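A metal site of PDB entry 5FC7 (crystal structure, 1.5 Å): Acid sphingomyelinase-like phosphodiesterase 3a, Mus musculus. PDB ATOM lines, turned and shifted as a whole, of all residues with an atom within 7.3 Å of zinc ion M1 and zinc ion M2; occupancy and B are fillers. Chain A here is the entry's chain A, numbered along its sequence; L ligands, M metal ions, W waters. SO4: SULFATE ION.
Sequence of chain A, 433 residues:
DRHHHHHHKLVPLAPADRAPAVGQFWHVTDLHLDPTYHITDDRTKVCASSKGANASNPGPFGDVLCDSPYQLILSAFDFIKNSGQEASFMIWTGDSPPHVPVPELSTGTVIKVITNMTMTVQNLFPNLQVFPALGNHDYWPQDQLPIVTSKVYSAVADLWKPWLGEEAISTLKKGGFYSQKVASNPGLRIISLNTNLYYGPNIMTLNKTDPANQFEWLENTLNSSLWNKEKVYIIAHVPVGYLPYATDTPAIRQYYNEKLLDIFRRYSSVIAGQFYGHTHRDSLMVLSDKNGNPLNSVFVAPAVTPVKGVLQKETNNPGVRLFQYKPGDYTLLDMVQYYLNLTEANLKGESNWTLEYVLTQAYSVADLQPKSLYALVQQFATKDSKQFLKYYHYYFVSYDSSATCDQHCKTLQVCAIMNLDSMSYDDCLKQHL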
ATOM      1  N   THR A  29      15.236 -11.178 -15.886  1.00  0.00           N
ATOM      2  CA  THR A  29      15.526  -9.772 -16.165  1.00  0.00           C
ATOM      3  C   THR A  29      16.286  -9.116 -15.024  1.00  0.00           C
ATOM      4  O   THR A  29      16.223  -9.531 -13.866  1.00  0.00           O
ATOM      5  CB  THR A  29      14.245  -8.995 -16.524  1.00  0.00           C
ATOM      6  OG1 THR A  29      14.565  -7.726 -17.134  1.00  0.00           O
ATOM      7  CG2 THR A  29      13.373  -8.785 -15.355  1.00  0.00           C
ATOM      8  N   ASP A  30      17.012  -8.070 -15.370  1.00  0.00           N
ATOM      9  CA  ASP A  30      17.622  -7.159 -14.408  1.00  0.00           C
ATOM     10  C   ASP A  30      18.479  -7.929 -13.395  1.00  0.00           C
ATOM     11  O   ASP A  30      18.254  -7.863 -12.184  1.00  0.00           O
ATOM     12  CB  ASP A  30      16.532  -6.304 -13.736  1.00  0.00           C
ATOM     13  CG  ASP A  30      15.922  -5.312 -14.702  1.00  0.00           C
ATOM     14  OD1 ASP A  30      16.478  -4.195 -14.786  1.00  0.00           O
ATOM     15  OD2 ASP A  30      14.900  -5.646 -15.383  1.00  0.00           O
ATOM     16  N   LEU A  31      19.462  -8.665 -13.946  1.00  0.00           N
ATOM     17  CA  LEU A  31      20.376  -9.460 -13.142  1.00  0.00           C
ATOM     18  C   LEU A  31      21.306  -8.583 -12.309  1.00  0.00           C
ATOM     19  O   LEU A  31      21.589  -8.885 -11.145  1.00  0.00           O
ATOM     20  CB  LEU A  31      21.175 -10.401 -14.050  1.00  0.00           C
ATOM     21  CG  LEU A  31      20.325 -11.406 -14.860  1.00  0.00           C
ATOM     22  CD1 LEU A  31      21.208 -12.269 -15.794  1.00  0.00           C
ATOM     23  CD2 LEU A  31      19.492 -12.320 -13.967  1.00  0.00           C
ATOM     24  N   HIS A  32      21.793  -7.492 -12.906  1.00  0.00           N
ATOM     25  CA  HIS A  32      22.643  -6.514 -12.234  1.00  0.00           C
ATOM     26  C   HIS A  32      23.693  -7.175 -11.345  1.00  0.00           C
ATOM     27  O   HIS A  32      23.728  -7.001 -10.126  1.00  0.00           O
ATOM     28  CB  HIS A  32      21.819  -5.515 -11.438  1.00  0.00           C
ATOM     29  CG  HIS A  32      20.964  -4.609 -12.264  1.00  0.00           C
ATOM     30  ND1 HIS A  32      21.459  -3.535 -12.970  1.00  0.00           N
ATOM     31  CD2 HIS A  32      19.618  -4.568 -12.412  1.00  0.00           C
ATOM     32  CE1 HIS A  32      20.454  -2.881 -13.533  1.00  0.00           C
ATOM     33  NE2 HIS A  32      19.326  -3.487 -13.195  1.00  0.00           N
ATOM     34  N   ASP A  67      23.573  -4.597  -5.368  1.00  0.00           N
ATOM     35  CA  ASP A  67      23.227  -5.423  -6.512  1.00  0.00           C
ATOM     36  C   ASP A  67      23.642  -6.870  -6.262  1.00  0.00           C
ATOM     37  O   ASP A  67      24.140  -7.238  -5.200  1.00  0.00           O
ATOM     38  CB  ASP A  67      23.800  -4.815  -7.762  1.00  0.00           C
ATOM     39  CG  ASP A  67      22.844  -3.838  -8.386  1.00  0.00           C
ATOM     40  OD1 ASP A  67      21.632  -4.129  -8.422  1.00  0.00           O
ATOM     41  OD2 ASP A  67      23.282  -2.745  -8.790  1.00  0.00           O
ATOM     42  N   THR A  93      15.525  -9.869 -20.472  1.00  0.00           N
ATOM     43  CA  THR A  93      15.277  -8.487 -20.884  1.00  0.00           C
ATOM     44  C   THR A  93      16.210  -7.442 -20.296  1.00  0.00           C
ATOM     45  O   THR A  93      15.781  -6.325 -20.005  1.00  0.00           O
ATOM     46  CB  THR A  93      13.804  -8.087 -20.702  1.00  0.00           C
ATOM     47  OG1 THR A  93      13.339  -8.486 -19.432  1.00  0.00           O
ATOM     48  CG2 THR A  93      12.943  -8.811 -21.718  1.00  0.00           C
ATOM     49  N   GLY A  94      17.503  -7.763 -20.145  1.00  0.00           N
ATOM     50  CA  GLY A  94      18.542  -6.755 -20.019  1.00  0.00           C
ATOM     51  C   GLY A  94      18.923  -6.353 -18.603  1.00  0.00           C
ATOM     52  O   GLY A  94      18.417  -6.862 -17.586  1.00  0.00           O
ATOM     53  N   ASP A  95      19.878  -5.420 -18.554  1.00  0.00           N
ATOM     54  CA  ASP A  95      20.395  -4.771 -17.338  1.00  0.00           C
ATOM     55  C   ASP A  95      21.327  -5.658 -16.537  1.00  0.00           C
ATOM     56  O   ASP A  95      21.014  -6.081 -15.406  1.00  0.00           O
ATOM     57  CB  ASP A  95      19.289  -4.190 -16.481  1.00  0.00           C
ATOM     58  CG  ASP A  95      19.123  -2.673 -16.665  1.00  0.00           C
ATOM     59  OD1 ASP A  95      19.680  -2.116 -17.610  1.00  0.00           O
ATOM     60  OD2 ASP A  95      18.387  -2.026 -15.875  1.00  0.00           O
ATOM     61  N   SER A  96      22.503  -5.883 -17.085  1.00  0.00           N
ATOM     62  CA  SER A  96      23.452  -6.796 -16.462  1.00  0.00           C
ATOM     63  C   SER A  96      24.507  -6.140 -15.568  1.00  0.00           C
ATOM     64  O   SER A  96      24.818  -6.708 -14.527  1.00  0.00           O
ATOM     65  CB  SER A  96      24.083  -7.707 -17.517  1.00  0.00           C
ATOM     66  OG  SER A  96      23.098  -8.597 -18.042  1.00  0.00           O
ATOM     67  N   PRO A  97      25.082  -4.996 -15.912  1.00  0.00           N
ATOM     68  CA  PRO A  97      26.063  -4.370 -15.001  1.00  0.00           C
ATOM     69  C   PRO A  97      25.385  -3.741 -13.790  1.00  0.00           C
ATOM     70  O   PRO A  97      24.178  -3.487 -13.787  1.00  0.00           O
ATOM     71  CB  PRO A  97      26.702  -3.285 -15.883  1.00  0.00           C
ATOM     72  CG  PRO A  97      26.380  -3.669 -17.284  1.00  0.00           C
ATOM     73  CD  PRO A  97      25.031  -4.300 -17.203  1.00  0.00           C
ATOM     74  N   HIS A  99      24.645  -0.982 -10.489  1.00  0.00           N
ATOM     75  CA  HIS A  99      24.391   0.445 -10.279  1.00  0.00           C
ATOM     76  C   HIS A  99      25.579   0.992  -9.517  1.00  0.00           C
ATOM     77  O   HIS A  99      25.593   1.093  -8.285  1.00  0.00           O
ATOM     78  CB  HIS A  99      23.111   0.659  -9.473  1.00  0.00           C
ATOM     79  CG  HIS A  99      21.870   0.129 -10.135  1.00  0.00           C
ATOM     80  ND1 HIS A  99      21.515  -1.200 -10.064  1.00  0.00           N
ATOM     81  CD2 HIS A  99      20.947   0.720 -10.931  1.00  0.00           C
ATOM     82  CE1 HIS A  99      20.396  -1.386 -10.731  1.00  0.00           C
ATOM     83  NE2 HIS A  99      20.035  -0.246 -11.269  1.00  0.00           N
ATOM     84  N   GLY A 135      19.369  -3.642 -21.959  1.00  0.00           N
ATOM     85  CA  GLY A 135      18.851  -2.723 -20.958  1.00  0.00           C
ATOM     86  C   GLY A 135      19.625  -1.410 -20.939  1.00  0.00           C
ATOM     87  O   GLY A 135      20.665  -1.271 -21.595  1.00  0.00           O
ATOM     88  N   ASN A 136      19.110  -0.424 -20.184  1.00  0.00           N
ATOM     89  CA  ASN A 136      19.737   0.893 -20.205  1.00  0.00           C
ATOM     90  C   ASN A 136      21.111   0.871 -19.541  1.00  0.00           C
ATOM     91  O   ASN A 136      21.949   1.713 -19.881  1.00  0.00           O
ATOM     92  CB  ASN A 136      18.841   1.972 -19.577  1.00  0.00           C
ATOM     93  CG  ASN A 136      18.341   1.598 -18.209  1.00  0.00           C
ATOM     94  OD1 ASN A 136      17.626   0.610 -18.056  1.00  0.00           O
ATOM     95  ND2 ASN A 136      18.721   2.369 -17.198  1.00  0.00           N
ATOM     96  N   HIS A 137      21.382  -0.084 -18.630  1.00  0.00           N
ATOM     97  CA  HIS A 137      22.701  -0.225 -18.055  1.00  0.00           C
ATOM     98  C   HIS A 137      23.645  -1.041 -18.937  1.00  0.00           C
ATOM     99  O   HIS A 137      24.850  -1.126 -18.626  1.00  0.00           O
ATOM    100  CB  HIS A 137      22.648  -0.837 -16.657  1.00  0.00           C
ATOM    101  CG  HIS A 137      22.071   0.069 -15.642  1.00  0.00           C
ATOM    102  ND1 HIS A 137      22.847   0.909 -14.872  1.00  0.00           N
ATOM    103  CD2 HIS A 137      20.780   0.332 -15.324  1.00  0.00           C
ATOM    104  CE1 HIS A 137      22.060   1.620 -14.094  1.00  0.00           C
ATOM    105  NE2 HIS A 137      20.805   1.284 -14.334  1.00  0.00           N
ATOM    106  N   ASP A 143      22.586   4.458 -20.151  1.00  0.00           N
ATOM    107  CA  ASP A 143      21.444   5.146 -20.730  1.00  0.00           C
ATOM    108  C   ASP A 143      21.721   5.754 -22.099  1.00  0.00           C
ATOM    109  O   ASP A 143      20.774   6.122 -22.781  1.00  0.00           O
ATOM    110  CB  ASP A 143      20.880   6.251 -19.814  1.00  0.00           C
ATOM    111  CG  ASP A 143      20.617   5.771 -18.398  1.00  0.00           C
ATOM    112  OD1 ASP A 143      20.323   4.578 -18.220  1.00  0.00           O
ATOM    113  OD2 ASP A 143      20.700   6.606 -17.457  1.00  0.00           O
ATOM    114  N   ASN A 196      15.388   1.486 -24.920  1.00  0.00           N
ATOM    115  CA  ASN A 196      16.278   2.462 -24.298  1.00  0.00           C
ATOM    116  C   ASN A 196      16.505   3.652 -25.227  1.00  0.00           C
ATOM    117  O   ASN A 196      16.915   4.715 -24.760  1.00  0.00           O
ATOM    118  CB  ASN A 196      17.600   1.789 -23.958  1.00  0.00           C
ATOM    119  CG  ASN A 196      17.408   0.503 -23.215  1.00  0.00           C
ATOM    120  OD1 ASN A 196      16.983   0.491 -22.058  1.00  0.00           O
ATOM    121  ND2 ASN A 196      17.677  -0.602 -23.883  1.00  0.00           N
ATOM    122  N   TYR A 199      14.065   6.159 -23.746  1.00  0.00           N
ATOM    123  CA  TYR A 199      14.116   6.390 -22.325  1.00  0.00           C
ATOM    124  C   TYR A 199      14.631   7.797 -22.066  1.00  0.00           C
ATOM    125  O   TYR A 199      15.592   8.269 -22.714  1.00  0.00           O
ATOM    126  CB  TYR A 199      15.068   5.331 -21.777  1.00  0.00           C
ATOM    127  CG  TYR A 199      15.237   5.283 -20.283  1.00  0.00           C
ATOM    128  CD1 TYR A 199      14.162   5.366 -19.424  1.00  0.00           C
ATOM    129  CD2 TYR A 199      16.507   5.150 -19.730  1.00  0.00           C
ATOM    130  CE1 TYR A 199      14.344   5.319 -18.022  1.00  0.00           C
ATOM    131  CE2 TYR A 199      16.727   5.056 -18.370  1.00  0.00           C
ATOM    132  CZ  TYR A 199      15.631   5.164 -17.506  1.00  0.00           C
ATOM    133  OH  TYR A 199      15.801   5.141 -16.119  1.00  0.00           O
ATOM    134  N   HIS A 237      13.404  -3.993 -22.634  1.00  0.00           N
ATOM    135  CA  HIS A 237      13.778  -3.637 -21.269  1.00  0.00           C
ATOM    136  C   HIS A 237      12.770  -2.657 -20.662  1.00  0.00           C
ATOM    137  O   HIS A 237      11.965  -3.044 -19.818  1.00  0.00           O
ATOM    138  CB  HIS A 237      15.212  -3.097 -21.211  1.00  0.00           C
ATOM    139  CG  HIS A 237      15.639  -2.778 -19.810  1.00  0.00           C
ATOM    140  ND1 HIS A 237      15.811  -3.748 -18.854  1.00  0.00           N
ATOM    141  CD2 HIS A 237      15.911  -1.593 -19.192  1.00  0.00           C
ATOM    142  CE1 HIS A 237      16.177  -3.192 -17.711  1.00  0.00           C
ATOM    143  NE2 HIS A 237      16.244  -1.880 -17.888  1.00  0.00           N
ATOM    144  N   VAL A 238      12.772  -1.405 -21.123  1.00  0.00           N
ATOM    145  CA  VAL A 238      11.881  -0.402 -20.562  1.00  0.00           C
ATOM    146  C   VAL A 238      10.479  -0.621 -21.129  1.00  0.00           C
ATOM    147  O   VAL A 238      10.314  -0.702 -22.364  1.00  0.00           O
ATOM    148  CB  VAL A 238      12.383   1.013 -20.885  1.00  0.00           C
ATOM    149  CG1 VAL A 238      11.528   2.027 -20.112  1.00  0.00           C
ATOM    150  CG2 VAL A 238      13.858   1.159 -20.590  1.00  0.00           C
ATOM    151  N   GLY A 277      10.987  -5.522 -18.527  1.00  0.00           N
ATOM    152  CA  GLY A 277      11.662  -5.465 -17.231  1.00  0.00           C
ATOM    153  C   GLY A 277      11.780  -4.029 -16.740  1.00  0.00           C
ATOM    154  O   GLY A 277      10.788  -3.273 -16.783  1.00  0.00           O
ATOM    155  N   HIS A 278      12.983  -3.656 -16.292  1.00  0.00           N
ATOM    156  CA  HIS A 278      13.388  -2.298 -15.911  1.00  0.00           C
ATOM    157  C   HIS A 278      12.821  -1.777 -14.590  1.00  0.00           C
ATOM    158  O   HIS A 278      13.552  -1.137 -13.832  1.00  0.00           O
ATOM    159  CB  HIS A 278      13.077  -1.321 -17.030  1.00  0.00           C
ATOM    160  CG  HIS A 278      13.462   0.088 -16.740  1.00  0.00           C
ATOM    161  ND1 HIS A 278      14.770   0.499 -16.646  1.00  0.00           N
ATOM    162  CD2 HIS A 278      12.697   1.186 -16.513  1.00  0.00           C
ATOM    163  CE1 HIS A 278      14.801   1.794 -16.342  1.00  0.00           C
ATOM    164  NE2 HIS A 278      13.549   2.238 -16.293  1.00  0.00           N
ATOM    165  N   THR A 279      11.535  -2.008 -14.311  1.00  0.00           N
ATOM    166  CA  THR A 279      10.947  -1.438 -13.101  1.00  0.00           C
ATOM    167  C   THR A 279      11.326  -2.192 -11.842  1.00  0.00           C
ATOM    168  O   THR A 279      11.173  -1.633 -10.735  1.00  0.00           O
ATOM    169  CB  THR A 279       9.433  -1.376 -13.201  1.00  0.00           C
ATOM    170  OG1 THR A 279       8.909  -2.687 -13.101  1.00  0.00           O
ATOM    171  CG2 THR A 279       8.979  -0.690 -14.517  1.00  0.00           C
ATOM    172  N   HIS A 280      11.831  -3.425 -11.980  1.00  0.00           N
ATOM    173  CA  HIS A 280      12.191  -4.292 -10.872  1.00  0.00           C
ATOM    174  C   HIS A 280      10.970  -4.677 -10.015  1.00  0.00           C
ATOM    175  O   HIS A 280      11.128  -5.071  -8.863  1.00  0.00           O
ATOM    176  CB  HIS A 280      13.292  -3.717  -9.983  1.00  0.00           C
ATOM    177  CG  HIS A 280      14.619  -3.461 -10.654  1.00  0.00           C
ATOM    178  ND1 HIS A 280      15.762  -3.239  -9.912  1.00  0.00           N
ATOM    179  CD2 HIS A 280      14.993  -3.387 -11.954  1.00  0.00           C
ATOM    180  CE1 HIS A 280      16.786  -3.050 -10.741  1.00  0.00           C
ATOM    181  NE2 HIS A 280      16.338  -3.138 -11.982  1.00  0.00           N
ATOM    182  N   ALA A 303      12.916  -8.027 -10.864  1.00  0.00           N
ATOM    183  CA  ALA A 303      14.330  -8.242 -11.039  1.00  0.00           C
ATOM    184  C   ALA A 303      14.851  -9.407 -10.193  1.00  0.00           C
ATOM    185  O   ALA A 303      14.256  -9.814  -9.184  1.00  0.00           O
ATOM    186  CB  ALA A 303      15.084  -6.994 -10.600  1.00  0.00           C
ATOM    187  N   THR A 305      18.049  -8.775  -8.967  1.00  0.00           N
ATOM    188  CA  THR A 305      18.647  -7.924  -7.942  1.00  0.00           C
ATOM    189  C   THR A 305      17.578  -7.407  -6.982  1.00  0.00           C
ATOM    190  O   THR A 305      16.447  -7.065  -7.413  1.00  0.00           O
ATOM    191  CB  THR A 305      19.398  -6.735  -8.540  1.00  0.00           C
ATOM    192  OG1 THR A 305      20.053  -6.008  -7.482  1.00  0.00           O
ATOM    193  CG2 THR A 305      18.451  -5.781  -9.302  1.00  0.00           C
ATOM    194  N   VAL A 307      18.258  -4.625  -5.174  1.00  0.00           N
ATOM    195  CA  VAL A 307      18.844  -3.332  -4.802  1.00  0.00           C
ATOM    196  C   VAL A 307      17.787  -2.251  -4.611  1.00  0.00           C
ATOM    197  O   VAL A 307      16.796  -2.170  -5.350  1.00  0.00           O
ATOM    198  CB  VAL A 307      19.892  -2.918  -5.857  1.00  0.00           C
ATOM    199  CG1 VAL A 307      19.221  -2.488  -7.184  1.00  0.00           C
ATOM    200  CG2 VAL A 307      20.817  -1.842  -5.326  1.00  0.00           C
HETATM  201  S   SO4 L   1      17.389   0.673 -13.649  1.00  0.00           S
HETATM  202  O1  SO4 L   1      16.080   1.039 -13.035  1.00  0.00           O
HETATM  203  O2  SO4 L   1      18.327   1.740 -13.136  1.00  0.00           O
HETATM  204  O3  SO4 L   1      17.946  -0.595 -13.139  1.00  0.00           O
HETATM  205  O4  SO4 L   1      17.456   0.788 -15.117  1.00  0.00           O
HETATM  206 ZN    ZN M   1      17.457  -2.721 -13.801  1.00  0.00          ZN
HETATM  207 ZN    ZN M   2      16.728  -0.477 -16.550  1.00  0.00          ZN
HETATM  208  O   HOH W   1      16.204  -1.407 -14.517  1.00  0.00           O
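Zinc ion M1 is bound by water W1 (2.0 Å), OD1 of Asp 30 (2.0 Å), NE2 of His 32 (2.1 Å), NE2 of His 280 (2.2 Å), O3 of the ligand (2.3 Å) and OD2 of Asp 95 (2.4 Å).
Zinc ion M1 has six donor atoms within binding distance.
Four residues have an atom within 4 Å of zinc ion M1: Asp 30, His 32, Asp 95 and His 280.
Along chain A the residues within 4 Å of zinc ion M1 span positions 30 to 280.
The nearest printed residue that does not touch zinc ion M1 is His 237 (4.1 Å).
The backbone NH (N) of Asp 30 is in hydrogen-bond range of the backbone carbonyl oxygen (O) of Gly 94 (2.9 Å).
The backbone carbonyl oxygen (O) of Asp 30 sits at hydrogen-bond distance from the backbone NH (N) of Thr 305 (3.4 Å).
The side-chain carboxylate (OD2) of Asp 30 sits at hydrogen-bond distance from the backbone NH (N) of His 278, at 2.9 Å.
OD1 of Asp 95 sits at hydrogen-bond distance from N of His 137, at 2.8 Å.
The side-chain hydroxyl (OG1) of Thr 29 lies within hydrogen-bond range of the side-chain carboxylate (OD2) of Asp 30, 2.7 Å away.
The side-chain amide oxygen of Asn 196 is in hydrogen-bond range of the backbone NH of Asn 136 (3.0 Å).
A ring nitrogen (ND1) of His 237 sits at hydrogen-bond distance from the backbone carbonyl oxygen (O) of Thr 93 (2.8 Å).
O of His 237 sits at hydrogen-bond distance from N of Gly 277.
Zinc ion M2 is bound by a ring nitrogen (NE2) of His 237, an oxygen (O4) of the ligand, the side-chain amide oxygen (OD1) of Asn 136, a ring nitrogen (ND1) of His 278, water W1 and the side-chain carboxylate (OD2) of Asp 95.
Zinc ion M2 has six donor atoms within binding distance.
The nearest printed residue that does not touch zinc ion M2 is Asp 30 (4.1 Å).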
